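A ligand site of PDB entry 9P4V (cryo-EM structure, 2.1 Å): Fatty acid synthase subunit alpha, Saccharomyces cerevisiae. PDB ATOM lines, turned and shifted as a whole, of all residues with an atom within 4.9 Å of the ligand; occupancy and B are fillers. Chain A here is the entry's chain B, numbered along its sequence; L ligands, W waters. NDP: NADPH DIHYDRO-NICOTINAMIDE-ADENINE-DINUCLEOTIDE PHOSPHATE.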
ATOM      1  N   GLY A 682       1.992 -17.653  27.433  1.00  0.00           N
ATOM      2  CA  GLY A 682       2.385 -17.176  26.119  1.00  0.00           C
ATOM      3  C   GLY A 682       3.179 -15.883  26.085  1.00  0.00           C
ATOM      4  O   GLY A 682       3.083 -15.136  25.126  1.00  0.00           O
ATOM      5  N   GLY A 684       6.574 -15.499  26.039  1.00  0.00           N
ATOM      6  CA  GLY A 684       7.958 -15.724  25.697  1.00  0.00           C
ATOM      7  C   GLY A 684       8.611 -14.578  24.976  1.00  0.00           C
ATOM      8  O   GLY A 684       7.940 -13.644  24.542  1.00  0.00           O
ATOM      9  N   SER A 687       7.229 -11.774  22.039  1.00  0.00           N
ATOM     10  CA  SER A 687       5.766 -11.807  22.005  1.00  0.00           C
ATOM     11  C   SER A 687       5.156 -10.561  22.608  1.00  0.00           C
ATOM     12  O   SER A 687       5.841  -9.796  23.266  1.00  0.00           O
ATOM     13  CB  SER A 687       5.266 -13.002  22.803  1.00  0.00           C
ATOM     14  OG  SER A 687       5.309 -12.753  24.189  1.00  0.00           O
ATOM     15  N   ILE A 688       3.867 -10.360  22.391  1.00  0.00           N
ATOM     16  CA  ILE A 688       3.172  -9.246  23.024  1.00  0.00           C
ATOM     17  C   ILE A 688       3.158  -9.499  24.517  1.00  0.00           C
ATOM     18  O   ILE A 688       3.267  -8.574  25.304  1.00  0.00           O
ATOM     19  CB  ILE A 688       1.738  -9.084  22.501  1.00  0.00           C
ATOM     20  CG1 ILE A 688       1.743  -8.801  21.002  1.00  0.00           C
ATOM     21  CG2 ILE A 688       1.013  -7.962  23.243  1.00  0.00           C
ATOM     22  CD1 ILE A 688       0.386  -8.917  20.333  1.00  0.00           C
ATOM     23  N   GLY A 689       3.040 -10.764  24.901  1.00  0.00           N
ATOM     24  CA  GLY A 689       2.994 -11.117  26.293  1.00  0.00           C
ATOM     25  C   GLY A 689       4.228 -10.724  27.068  1.00  0.00           C
ATOM     26  O   GLY A 689       4.115 -10.305  28.203  1.00  0.00           O
ATOM     27  N   THR A 706       4.144 -18.584  32.604  1.00  0.00           N
ATOM     28  CA  THR A 706       4.368 -19.947  32.166  1.00  0.00           C
ATOM     29  C   THR A 706       5.286 -20.022  30.975  1.00  0.00           C
ATOM     30  O   THR A 706       5.555 -19.022  30.339  1.00  0.00           O
ATOM     31  CB  THR A 706       3.021 -20.615  31.807  1.00  0.00           C
ATOM     32  OG1 THR A 706       2.441 -19.954  30.668  1.00  0.00           O
ATOM     33  CG2 THR A 706       2.052 -20.560  32.967  1.00  0.00           C
ATOM     34  N   THR A 707       5.799 -21.201  30.675  1.00  0.00           N
ATOM     35  CA  THR A 707       6.636 -21.378  29.505  1.00  0.00           C
ATOM     36  C   THR A 707       6.564 -22.806  29.021  1.00  0.00           C
ATOM     37  O   THR A 707       6.557 -23.733  29.823  1.00  0.00           O
ATOM     38  CB  THR A 707       8.124 -21.007  29.768  1.00  0.00           C
ATOM     39  OG1 THR A 707       8.882 -21.195  28.575  1.00  0.00           O
ATOM     40  CG2 THR A 707       8.714 -21.867  30.874  1.00  0.00           C
ATOM     41  N   SER A 708       6.536 -22.975  27.726  1.00  0.00           N
ATOM     42  CA  SER A 708       6.475 -24.291  27.123  1.00  0.00           C
ATOM     43  C   SER A 708       7.882 -24.766  26.767  1.00  0.00           C
ATOM     44  O   SER A 708       8.059 -25.910  26.387  1.00  0.00           O
ATOM     45  CB  SER A 708       5.538 -24.265  25.891  1.00  0.00           C
ATOM     46  OG  SER A 708       6.040 -23.429  24.879  1.00  0.00           O
ATOM     47  N   ARG A 709       8.890 -23.911  26.909  1.00  0.00           N
ATOM     48  CA  ARG A 709      10.295 -24.287  26.635  1.00  0.00           C
ATOM     49  C   ARG A 709      11.202 -24.032  27.831  1.00  0.00           C
ATOM     50  O   ARG A 709      12.176 -23.316  27.718  1.00  0.00           O
ATOM     51  CB  ARG A 709      10.811 -23.528  25.421  1.00  0.00           C
ATOM     52  CG  ARG A 709       9.957 -23.641  24.189  1.00  0.00           C
ATOM     53  CD  ARG A 709      10.487 -22.733  23.090  1.00  0.00           C
ATOM     54  NE  ARG A 709      10.505 -21.336  23.508  1.00  0.00           N
ATOM     55  CZ  ARG A 709      11.555 -20.694  24.018  1.00  0.00           C
ATOM     56  NH1 ARG A 709      11.446 -19.418  24.359  1.00  0.00           N
ATOM     57  NH2 ARG A 709      12.718 -21.317  24.201  1.00  0.00           N
ATOM     58  N   PHE A 737       4.959 -25.233  31.630  1.00  0.00           N
ATOM     59  CA  PHE A 737       3.525 -25.375  31.449  1.00  0.00           C
ATOM     60  C   PHE A 737       3.249 -25.817  30.029  1.00  0.00           C
ATOM     61  O   PHE A 737       3.833 -25.290  29.082  1.00  0.00           O
ATOM     62  CB  PHE A 737       2.828 -24.048  31.725  1.00  0.00           C
ATOM     63  CG  PHE A 737       1.332 -24.121  31.729  1.00  0.00           C
ATOM     64  CD1 PHE A 737       0.662 -24.979  32.573  1.00  0.00           C
ATOM     65  CD2 PHE A 737       0.594 -23.296  30.895  1.00  0.00           C
ATOM     66  CE1 PHE A 737      -0.719 -25.021  32.576  1.00  0.00           C
ATOM     67  CE2 PHE A 737      -0.786 -23.338  30.898  1.00  0.00           C
ATOM     68  CZ  PHE A 737      -1.442 -24.195  31.739  1.00  0.00           C
ATOM     69  N   ASN A 738       2.359 -26.790  29.885  1.00  0.00           N
ATOM     70  CA  ASN A 738       1.800 -27.148  28.589  1.00  0.00           C
ATOM     71  C   ASN A 738       0.307 -26.832  28.660  1.00  0.00           C
ATOM     72  O   ASN A 738      -0.463 -27.599  29.238  1.00  0.00           O
ATOM     73  CB  ASN A 738       2.054 -28.621  28.283  1.00  0.00           C
ATOM     74  CG  ASN A 738       1.420 -29.070  26.977  1.00  0.00           C
ATOM     75  OD1 ASN A 738       1.042 -28.259  26.144  1.00  0.00           O
ATOM     76  ND2 ASN A 738       1.317 -30.361  26.801  1.00  0.00           N
ATOM     77  N   GLN A 739      -0.086 -25.693  28.103  1.00  0.00           N
ATOM     78  CA  GLN A 739      -1.492 -25.325  28.063  1.00  0.00           C
ATOM     79  C   GLN A 739      -2.331 -26.342  27.299  1.00  0.00           C
ATOM     80  O   GLN A 739      -3.543 -26.373  27.470  1.00  0.00           O
ATOM     81  CB  GLN A 739      -1.665 -23.942  27.442  1.00  0.00           C
ATOM     82  CG  GLN A 739      -3.069 -23.336  27.592  1.00  0.00           C
ATOM     83  CD  GLN A 739      -3.092 -21.835  27.466  1.00  0.00           C
ATOM     84  OE1 GLN A 739      -2.416 -21.140  28.199  1.00  0.00           O
ATOM     85  NE2 GLN A 739      -3.857 -21.319  26.507  1.00  0.00           N
ATOM     86  N   GLY A 740      -1.699 -27.175  26.472  1.00  0.00           N
ATOM     87  CA  GLY A 740      -2.390 -28.240  25.771  1.00  0.00           C
ATOM     88  C   GLY A 740      -2.782 -29.434  26.621  1.00  0.00           C
ATOM     89  O   GLY A 740      -3.499 -30.311  26.140  1.00  0.00           O
ATOM     90  N   PRO A 770      -4.416 -15.379  29.112  1.00  0.00           N
ATOM     91  CA  PRO A 770      -4.046 -16.627  28.426  1.00  0.00           C
ATOM     92  C   PRO A 770      -3.714 -16.439  26.943  1.00  0.00           C
ATOM     93  O   PRO A 770      -4.516 -16.654  26.041  1.00  0.00           O
ATOM     94  CB  PRO A 770      -5.291 -17.498  28.609  1.00  0.00           C
ATOM     95  CG  PRO A 770      -6.408 -16.506  28.657  1.00  0.00           C
ATOM     96  CD  PRO A 770      -5.880 -15.222  29.197  1.00  0.00           C
ATOM     97  N   PHE A 771      -2.503 -15.978  26.687  1.00  0.00           N
ATOM     98  CA  PHE A 771      -2.099 -15.670  25.318  1.00  0.00           C
ATOM     99  C   PHE A 771      -1.331 -16.792  24.600  1.00  0.00           C
ATOM    100  O   PHE A 771      -0.953 -16.626  23.457  1.00  0.00           O
ATOM    101  CB  PHE A 771      -1.246 -14.406  25.341  1.00  0.00           C
ATOM    102  CG  PHE A 771      -2.038 -13.130  25.445  1.00  0.00           C
ATOM    103  CD1 PHE A 771      -3.344 -13.124  25.933  1.00  0.00           C
ATOM    104  CD2 PHE A 771      -1.480 -11.927  25.063  1.00  0.00           C
ATOM    105  CE1 PHE A 771      -4.066 -11.956  26.017  1.00  0.00           C
ATOM    106  CE2 PHE A 771      -2.194 -10.749  25.153  1.00  0.00           C
ATOM    107  CZ  PHE A 771      -3.489 -10.764  25.623  1.00  0.00           C
ATOM    108  N   ALA A 772      -1.124 -17.924  25.258  1.00  0.00           N
ATOM    109  CA  ALA A 772      -0.446 -19.038  24.615  1.00  0.00           C
ATOM    110  C   ALA A 772      -1.143 -19.438  23.319  1.00  0.00           C
ATOM    111  O   ALA A 772      -2.361 -19.477  23.243  1.00  0.00           O
ATOM    112  CB  ALA A 772      -0.368 -20.235  25.554  1.00  0.00           C
ATOM    113  N   ALA A 773      -0.354 -19.727  22.293  1.00  0.00           N
ATOM    114  CA  ALA A 773      -0.895 -20.145  21.007  1.00  0.00           C
ATOM    115  C   ALA A 773       0.177 -20.861  20.219  1.00  0.00           C
ATOM    116  O   ALA A 773       1.345 -20.766  20.557  1.00  0.00           O
ATOM    117  CB  ALA A 773      -1.387 -18.946  20.242  1.00  0.00           C
ATOM    118  N   ILE A 774      -0.214 -21.579  19.178  1.00  0.00           N
ATOM    119  CA  ILE A 774       0.763 -22.236  18.313  1.00  0.00           C
ATOM    120  C   ILE A 774       0.410 -21.929  16.872  1.00  0.00           C
ATOM    121  O   ILE A 774      -0.762 -21.845  16.536  1.00  0.00           O
ATOM    122  CB  ILE A 774       0.874 -23.757  18.548  1.00  0.00           C
ATOM    123  CG1 ILE A 774      -0.456 -24.456  18.279  1.00  0.00           C
ATOM    124  CG2 ILE A 774       1.326 -24.022  19.978  1.00  0.00           C
ATOM    125  CD1 ILE A 774      -0.339 -25.964  18.286  1.00  0.00           C
ATOM    126  N   PHE A 790      -5.098 -30.009  18.176  1.00  0.00           N
ATOM    127  CA  PHE A 790      -4.317 -29.687  19.369  1.00  0.00           C
ATOM    128  C   PHE A 790      -4.237 -28.177  19.581  1.00  0.00           C
ATOM    129  O   PHE A 790      -4.425 -27.709  20.685  1.00  0.00           O
ATOM    130  CB  PHE A 790      -2.920 -30.304  19.271  1.00  0.00           C
ATOM    131  CG  PHE A 790      -2.057 -30.050  20.464  1.00  0.00           C
ATOM    132  CD1 PHE A 790      -2.343 -30.655  21.677  1.00  0.00           C
ATOM    133  CD2 PHE A 790      -0.975 -29.212  20.382  1.00  0.00           C
ATOM    134  CE1 PHE A 790      -1.559 -30.432  22.788  1.00  0.00           C
ATOM    135  CE2 PHE A 790      -0.178 -28.969  21.490  1.00  0.00           C
ATOM    136  CZ  PHE A 790      -0.467 -29.584  22.689  1.00  0.00           C
ATOM    137  N   ILE A 794      -5.492 -25.944  22.872  1.00  0.00           N
ATOM    138  CA  ILE A 794      -4.722 -24.928  23.596  1.00  0.00           C
ATOM    139  C   ILE A 794      -5.471 -23.610  23.644  1.00  0.00           C
ATOM    140  O   ILE A 794      -5.617 -22.991  24.694  1.00  0.00           O
ATOM    141  CB  ILE A 794      -3.334 -24.731  22.963  1.00  0.00           C
ATOM    142  CG1 ILE A 794      -2.396 -25.899  23.283  1.00  0.00           C
ATOM    143  CG2 ILE A 794      -2.713 -23.415  23.442  1.00  0.00           C
ATOM    144  CD1 ILE A 794      -1.220 -25.953  22.383  1.00  0.00           C
ATOM    145  N   MET A 795      -5.958 -23.158  22.487  1.00  0.00           N
ATOM    146  CA  MET A 795      -6.377 -21.783  22.347  1.00  0.00           C
ATOM    147  C   MET A 795      -7.846 -21.549  22.674  1.00  0.00           C
ATOM    148  O   MET A 795      -8.247 -20.396  22.784  1.00  0.00           O
ATOM    149  CB  MET A 795      -6.068 -21.286  20.938  1.00  0.00           C
ATOM    150  CG  MET A 795      -4.588 -21.061  20.742  1.00  0.00           C
ATOM    151  SD  MET A 795      -3.933 -21.487  19.136  1.00  0.00           S
ATOM    152  CE  MET A 795      -4.378 -20.007  18.265  1.00  0.00           C
ATOM    153  N   PRO A 825      -7.554 -12.887  24.331  1.00  0.00           N
ATOM    154  CA  PRO A 825      -6.936 -12.417  23.090  1.00  0.00           C
ATOM    155  C   PRO A 825      -7.821 -12.731  21.895  1.00  0.00           C
ATOM    156  O   PRO A 825      -7.894 -13.868  21.426  1.00  0.00           O
ATOM    157  CB  PRO A 825      -5.626 -13.196  23.043  1.00  0.00           C
ATOM    158  CG  PRO A 825      -5.955 -14.487  23.708  1.00  0.00           C
ATOM    159  CD  PRO A 825      -7.077 -14.233  24.690  1.00  0.00           C
ATOM    160  N   MET A 826      -8.562 -11.738  21.421  1.00  0.00           N
ATOM    161  CA  MET A 826      -9.506 -11.944  20.344  1.00  0.00           C
ATOM    162  C   MET A 826      -8.974 -11.424  19.030  1.00  0.00           C
ATOM    163  O   MET A 826      -8.058 -10.610  19.013  1.00  0.00           O
ATOM    164  CB  MET A 826     -10.820 -11.247  20.676  1.00  0.00           C
ATOM    165  CG  MET A 826     -11.528 -11.909  21.838  1.00  0.00           C
ATOM    166  SD  MET A 826     -13.113 -11.167  22.256  1.00  0.00           S
ATOM    167  CE  MET A 826     -13.645 -12.306  23.523  1.00  0.00           C
ATOM    168  N   SER A 827      -9.531 -11.904  17.931  1.00  0.00           N
ATOM    169  CA  SER A 827      -9.056 -11.515  16.617  1.00  0.00           C
ATOM    170  C   SER A 827     -10.146 -10.776  15.853  1.00  0.00           C
ATOM    171  O   SER A 827     -11.320 -11.095  15.983  1.00  0.00           O
ATOM    172  CB  SER A 827      -8.614 -12.742  15.845  1.00  0.00           C
ATOM    173  OG  SER A 827      -8.633 -12.510  14.448  1.00  0.00           O
ATOM    174  N   PRO A 828      -9.748  -9.802  15.037  1.00  0.00           N
ATOM    175  CA  PRO A 828     -10.733  -9.071  14.230  1.00  0.00           C
ATOM    176  C   PRO A 828     -11.075  -9.735  12.906  1.00  0.00           C
ATOM    177  O   PRO A 828     -11.993  -9.284  12.250  1.00  0.00           O
ATOM    178  CB  PRO A 828     -10.022  -7.757  13.963  1.00  0.00           C
ATOM    179  CG  PRO A 828      -8.585  -8.144  13.870  1.00  0.00           C
ATOM    180  CD  PRO A 828      -8.399  -9.220  14.898  1.00  0.00           C
ATOM    181  N   TYR A 839      -7.538 -21.719  13.778  1.00  0.00           N
ATOM    182  CA  TYR A 839      -7.300 -20.481  14.496  1.00  0.00           C
ATOM    183  C   TYR A 839      -8.534 -19.621  14.588  1.00  0.00           C
ATOM    184  O   TYR A 839      -8.912 -19.176  15.661  1.00  0.00           O
ATOM    185  CB  TYR A 839      -6.200 -19.678  13.809  1.00  0.00           C
ATOM    186  CG  TYR A 839      -5.930 -18.338  14.431  1.00  0.00           C
ATOM    187  CD1 TYR A 839      -5.027 -18.203  15.460  1.00  0.00           C
ATOM    188  CD2 TYR A 839      -6.591 -17.195  13.995  1.00  0.00           C
ATOM    189  CE1 TYR A 839      -4.766 -16.983  16.040  1.00  0.00           C
ATOM    190  CE2 TYR A 839      -6.347 -15.966  14.566  1.00  0.00           C
ATOM    191  CZ  TYR A 839      -5.430 -15.860  15.591  1.00  0.00           C
ATOM    192  OH  TYR A 839      -5.177 -14.641  16.166  1.00  0.00           O
ATOM    193  N   LYS A 843     -10.730 -18.404  17.902  1.00  0.00           N
ATOM    194  CA  LYS A 843     -10.894 -16.989  18.236  1.00  0.00           C
ATOM    195  C   LYS A 843     -12.347 -16.572  18.275  1.00  0.00           C
ATOM    196  O   LYS A 843     -12.758 -15.876  19.182  1.00  0.00           O
ATOM    197  CB  LYS A 843     -10.130 -16.108  17.251  1.00  0.00           C
ATOM    198  CG  LYS A 843      -8.616 -16.245  17.358  1.00  0.00           C
ATOM    199  CD  LYS A 843      -8.101 -15.678  18.666  1.00  0.00           C
ATOM    200  CE  LYS A 843      -6.711 -16.169  18.972  1.00  0.00           C
ATOM    201  NZ  LYS A 843      -6.246 -15.703  20.307  1.00  0.00           N
ATOM    202  N   ILE A 869      -7.260  -7.668  19.219  1.00  0.00           N
ATOM    203  CA  ILE A 869      -5.900  -7.184  18.946  1.00  0.00           C
ATOM    204  C   ILE A 869      -5.637  -6.908  17.482  1.00  0.00           C
ATOM    205  O   ILE A 869      -5.896  -7.745  16.632  1.00  0.00           O
ATOM    206  CB  ILE A 869      -4.862  -8.203  19.488  1.00  0.00           C
ATOM    207  CG1 ILE A 869      -4.970  -8.287  21.000  1.00  0.00           C
ATOM    208  CG2 ILE A 869      -3.456  -7.827  19.078  1.00  0.00           C
ATOM    209  CD1 ILE A 869      -4.779  -9.689  21.550  1.00  0.00           C
ATOM    210  N   GLY A 870      -5.081  -5.736  17.203  1.00  0.00           N
ATOM    211  CA  GLY A 870      -4.826  -5.341  15.829  1.00  0.00           C
ATOM    212  C   GLY A 870      -3.516  -5.795  15.243  1.00  0.00           C
ATOM    213  O   GLY A 870      -2.798  -6.559  15.870  1.00  0.00           O
ATOM    214  N   TRP A 871      -3.219  -5.340  14.035  1.00  0.00           N
ATOM    215  CA  TRP A 871      -1.977  -5.705  13.364  1.00  0.00           C
ATOM    216  C   TRP A 871      -0.770  -5.333  14.205  1.00  0.00           C
ATOM    217  O   TRP A 871      -0.466  -4.169  14.357  1.00  0.00           O
ATOM    218  CB  TRP A 871      -1.943  -5.013  12.006  1.00  0.00           C
ATOM    219  CG  TRP A 871      -0.842  -5.408  11.102  1.00  0.00           C
ATOM    220  CD1 TRP A 871       0.495  -5.238  11.309  1.00  0.00           C
ATOM    221  CD2 TRP A 871      -0.977  -6.009   9.819  1.00  0.00           C
ATOM    222  NE1 TRP A 871       1.196  -5.718  10.239  1.00  0.00           N
ATOM    223  CE2 TRP A 871       0.310  -6.194   9.306  1.00  0.00           C
ATOM    224  CE3 TRP A 871      -2.076  -6.420   9.053  1.00  0.00           C
ATOM    225  CZ2 TRP A 871       0.545  -6.770   8.066  1.00  0.00           C
ATOM    226  CZ3 TRP A 871      -1.852  -6.996   7.830  1.00  0.00           C
ATOM    227  CH2 TRP A 871      -0.544  -7.171   7.340  1.00  0.00           C
ATOM    228  N   THR A 872      -0.086  -6.327  14.738  1.00  0.00           N
ATOM    229  CA  THR A 872       1.029  -6.077  15.638  1.00  0.00           C
ATOM    230  C   THR A 872       2.309  -6.601  14.987  1.00  0.00           C
ATOM    231  O   THR A 872       2.503  -7.807  14.894  1.00  0.00           O
ATOM    232  CB  THR A 872       0.820  -6.732  16.999  1.00  0.00           C
ATOM    233  OG1 THR A 872      -0.421  -6.286  17.567  1.00  0.00           O
ATOM    234  CG2 THR A 872       1.944  -6.372  17.941  1.00  0.00           C
ATOM    235  N   THR A 875       5.599 -10.367  15.849  1.00  0.00           N
ATOM    236  CA  THR A 875       5.316 -11.549  16.671  1.00  0.00           C
ATOM    237  C   THR A 875       5.480 -12.850  15.921  1.00  0.00           C
ATOM    238  O   THR A 875       5.760 -12.845  14.729  1.00  0.00           O
ATOM    239  CB  THR A 875       3.876 -11.516  17.231  1.00  0.00           C
ATOM    240  OG1 THR A 875       2.952 -11.461  16.135  1.00  0.00           O
ATOM    241  CG2 THR A 875       3.681 -10.307  18.135  1.00  0.00           C
ATOM    242  N   GLY A 876       5.294 -13.969  16.615  1.00  0.00           N
ATOM    243  CA  GLY A 876       5.357 -15.263  15.957  1.00  0.00           C
ATOM    244  C   GLY A 876       4.116 -15.455  15.111  1.00  0.00           C
ATOM    245  O   GLY A 876       4.098 -16.308  14.228  1.00  0.00           O
ATOM    246  N   LEU A 877       3.092 -14.643  15.361  1.00  0.00           N
ATOM    247  CA  LEU A 877       1.856 -14.756  14.624  1.00  0.00           C
ATOM    248  C   LEU A 877       1.766 -13.788  13.453  1.00  0.00           C
ATOM    249  O   LEU A 877       0.912 -13.944  12.580  1.00  0.00           O
ATOM    250  CB  LEU A 877       0.674 -14.513  15.571  1.00  0.00           C
ATOM    251  CG  LEU A 877      -0.728 -14.470  14.936  1.00  0.00           C
ATOM    252  CD1 LEU A 877      -1.018 -15.758  14.188  1.00  0.00           C
ATOM    253  CD2 LEU A 877      -1.809 -14.186  15.966  1.00  0.00           C
ATOM    254  N   MET A 878       2.655 -12.793  13.400  1.00  0.00           N
ATOM    255  CA  MET A 878       2.530 -11.786  12.348  1.00  0.00           C
ATOM    256  C   MET A 878       3.847 -11.330  11.713  1.00  0.00           C
ATOM    257  O   MET A 878       3.842 -10.532  10.797  1.00  0.00           O
ATOM    258  CB  MET A 878       1.786 -10.552  12.885  1.00  0.00           C
ATOM    259  CG  MET A 878       0.299 -10.757  13.054  1.00  0.00           C
ATOM    260  SD  MET A 878      -0.512 -11.036  11.474  1.00  0.00           S
ATOM    261  CE  MET A 878      -0.120  -9.513  10.618  1.00  0.00           C
HETATM  262  PA  NDP L   1       2.635 -15.948  19.809  1.00  0.00           P
HETATM  263  O1A NDP L   1       3.798 -16.483  19.020  1.00  0.00           O
HETATM  264  O2A NDP L   1       1.220 -16.247  19.382  1.00  0.00           O
HETATM  265  O5B NDP L   1       2.812 -16.438  21.318  1.00  0.00           O
HETATM  266  C5B NDP L   1       2.244 -17.661  21.775  1.00  0.00           C
HETATM  267  C4B NDP L   1       3.151 -18.137  22.888  1.00  0.00           C
HETATM  268  O4B NDP L   1       2.575 -19.242  23.575  1.00  0.00           O
HETATM  269  C3B NDP L   1       4.489 -18.631  22.353  1.00  0.00           C
HETATM  270  O3B NDP L   1       5.450 -17.576  22.355  1.00  0.00           O
HETATM  271  C2B NDP L   1       4.857 -19.753  23.290  1.00  0.00           C
HETATM  272  O2B NDP L   1       5.891 -19.304  24.147  1.00  0.00           O
HETATM  273  C1B NDP L   1       3.608 -20.080  24.083  1.00  0.00           C
HETATM  274  N9A NDP L   1       3.165 -21.476  23.915  1.00  0.00           N
HETATM  275  C8A NDP L   1       3.095 -22.157  22.761  1.00  0.00           C
HETATM  276  N7A NDP L   1       2.628 -23.417  22.987  1.00  0.00           N
HETATM  277  C5A NDP L   1       2.400 -23.541  24.311  1.00  0.00           C
HETATM  278  C6A NDP L   1       1.903 -24.587  25.219  1.00  0.00           C
HETATM  279  N6A NDP L   1       1.552 -25.809  24.772  1.00  0.00           N
HETATM  280  N1A NDP L   1       1.830 -24.289  26.525  1.00  0.00           N
HETATM  281  C2A NDP L   1       2.165 -23.088  27.021  1.00  0.00           C
HETATM  282  N3A NDP L   1       2.617 -22.094  26.249  1.00  0.00           N
HETATM  283  C4A NDP L   1       2.753 -22.251  24.911  1.00  0.00           C
HETATM  284  O3  NDP L   1       2.838 -14.366  19.968  1.00  0.00           O
HETATM  285  PN  NDP L   1       1.598 -13.357  20.107  1.00  0.00           P
HETATM  286  O1N NDP L   1       2.045 -12.187  20.945  1.00  0.00           O
HETATM  287  O2N NDP L   1       1.031 -13.124  18.736  1.00  0.00           O
HETATM  288  O5D NDP L   1       0.541 -14.191  20.979  1.00  0.00           O
HETATM  289  C5D NDP L   1      -0.565 -13.564  21.629  1.00  0.00           C
HETATM  290  C4D NDP L   1      -2.050 -13.887  21.578  1.00  0.00           C
HETATM  291  O4D NDP L   1      -2.787 -12.833  20.957  1.00  0.00           O
HETATM  292  C3D NDP L   1      -2.299 -15.144  20.761  1.00  0.00           C
HETATM  293  O3D NDP L   1      -3.218 -15.995  21.436  1.00  0.00           O
HETATM  294  C2D NDP L   1      -2.862 -14.642  19.455  1.00  0.00           C
HETATM  295  O2D NDP L   1      -3.759 -15.581  18.868  1.00  0.00           O
HETATM  296  C1D NDP L   1      -3.530 -13.336  19.841  1.00  0.00           C
HETATM  297  N1N NDP L   1      -3.544 -12.376  18.737  1.00  0.00           N
HETATM  298  C2N NDP L   1      -2.379 -11.924  18.245  1.00  0.00           C
HETATM  299  C3N NDP L   1      -2.356 -11.014  17.197  1.00  0.00           C
HETATM  300  C7N NDP L   1      -1.040 -10.509  16.643  1.00  0.00           C
HETATM  301  O7N NDP L   1      -1.026  -9.453  16.045  1.00  0.00           O
HETATM  302  N7N NDP L   1       0.067 -11.223  16.803  1.00  0.00           N
HETATM  303  C4N NDP L   1      -3.631 -10.499  16.576  1.00  0.00           C
HETATM  304  C5N NDP L   1      -4.821 -11.063  17.214  1.00  0.00           C
HETATM  305  C6N NDP L   1      -4.715 -11.971  18.256  1.00  0.00           C
HETATM  306  P2B NDP L   1       6.998 -20.262  24.789  1.00  0.00           P
HETATM  307  O1X NDP L   1       7.399 -21.197  23.686  1.00  0.00           O
HETATM  308  O2X NDP L   1       8.074 -19.278  25.169  1.00  0.00           O
HETATM  309  O3X NDP L   1       6.298 -20.893  25.956  1.00  0.00           O
HETATM  310  O   HOH W   1       1.549 -18.505  17.356  1.00  0.00           O
HETATM  311  O   HOH W   2      -0.843 -16.453  17.465  1.00  0.00           O
HETATM  312  O   HOH W   3      -6.076 -11.907  14.147  1.00  0.00           O
HETATM  313  O   HOH W   4       3.160 -26.594  22.396  1.00  0.00           O
HETATM  314  O   HOH W   5       1.906 -13.353  23.739  1.00  0.00           O
HETATM  315  O   HOH W   6       6.490 -14.708  19.932  1.00  0.00           O
HETATM  316  O   HOH W   7      -4.451 -17.732  23.535  1.00  0.00           O
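Water W7 lies within hydrogen-bond range of O of Pro 770, O of Ala 772 and O3D of the ligand.
Water W5 lies within hydrogen-bond range of the backbone carbonyl oxygen (O) of Gly 682 (2.5 Å), an oxygen (O1N) of the ligand (3.0 Å), the backbone NH (N) of Gly 689 (3.1 Å) and the side-chain hydroxyl (OG) of Ser 687 (3.5 Å).
The side-chain amide nitrogen of Gln 739 lies within hydrogen-bond range of the backbone carbonyl oxygen of Ile 794, 3.0 Å away.
The side-chain amino group of Lys 843 sits at hydrogen-bond distance from the backbone carbonyl oxygen of Pro 825, at 2.7 Å.
The backbone NH (N) of Arg 709 sits at hydrogen-bond distance from the side-chain hydroxyl (OG1) of Thr 707 (3.2 Å).
O of Gly 682 lies within hydrogen-bond range of OG of Ser 687.
N of Ile 774 is in hydrogen-bond range of SD of Met 795.
The backbone carbonyl oxygen of Thr 707 is in hydrogen-bond range of the backbone NH of Phe 737, at 2.8 Å.
O of Gly 870 sits at hydrogen-bond distance from OG1 of Thr 872 (2.9 Å).
The backbone carbonyl oxygen (O) of Gly 684 sits at hydrogen-bond distance from the side-chain hydroxyl (OG) of Ser 687 (2.8 Å).
An oxygen (O3X) of the ligand lies within hydrogen-bond range of the backbone NH of Ser 708 (2.7 Å).
The side-chain hydroxyl (OG) of Ser 708 is in hydrogen-bond range of an oxygen (O3X) of the ligand, 2.8 Å away.
The backbone NH (N) of Gln 739 is in hydrogen-bond range of a nitrogen (N1A) of the ligand.
A nitrogen (N6A) of the ligand is in hydrogen-bond range of the side-chain amide oxygen of Asn 738 (2.9 Å).
NZ of Lys 843 sits at hydrogen-bond distance from O2D of the ligand (2.9 Å).
O1N of the ligand is in hydrogen-bond range of N of Ile 688 (3.0 Å).
The side-chain hydroxyl (OG1) of Thr 875 lies within hydrogen-bond range of a nitrogen (N7N) of the ligand, at 3.0 Å.
The backbone carbonyl oxygen (O) of Phe 771 sits at hydrogen-bond distance from an oxygen (O3D) of the ligand, at 3.1 Å.
The guanidinium group of Arg 709 is in salt-bridge range of an oxygen (O1X) of the ligand (3.1 Å).
An oxygen (O4B) of the ligand is in hydrogen-bond range of the backbone NH (N) of Ala 773 (3.2 Å).
O2D of the ligand is in hydrogen-bond range of OH of Tyr 839 (3.2 Å).
A nitrogen (N1A) of the ligand sits close to the backbone carbonyl oxygen (O) of Phe 737.
The backbone carbonyl oxygen (O) of Gly 870 sits close to an oxygen (O7N) of the ligand (3.4 Å).
Merely in contact with the ligand: Gly 682 (3.3 Å), Gly 684 (3.6 Å), Ser 687 (3.8 Å), Thr 707 (3.6 Å), Gly 740 (3.9 Å), Ala 772 (3.2 Å), Ile 774 (3.3 Å), Ile 794 (3.7 Å), Pro 825 (3.5 Å), Met 826 (3.7 Å), Ile 869 (3.5 Å), Thr 872 (3.4 Å), Gly 876 (3.6 Å), Leu 877 (3.3 Å) and Met 878 (3.5 Å).
Hydrophobic or aromatic side chains that line the ligand: Ile 688, Phe 771, Ala 772, Ala 773, Ile 774, Ile 794, Pro 825, Tyr 839, Ile 869, Leu 877 and Met 878.
Within 4 Å of the ligand: Gly 682, Gly 684, Ser 687, Ile 688, Thr 707, Ser 708, Arg 709, Phe 737, Asn 738, Gln 739, Gly 740, Phe 771, Ala 772, Ala 773, Ile 774, Ile 794, Pro 825, Met 826, Tyr 839, Lys 843, Ile 869, Gly 870, Thr 872, Thr 875, Gly 876, Leu 877 and Met 878.
The nearest printed residue that does not touch the ligand is Ser 827 (4.3 Å).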
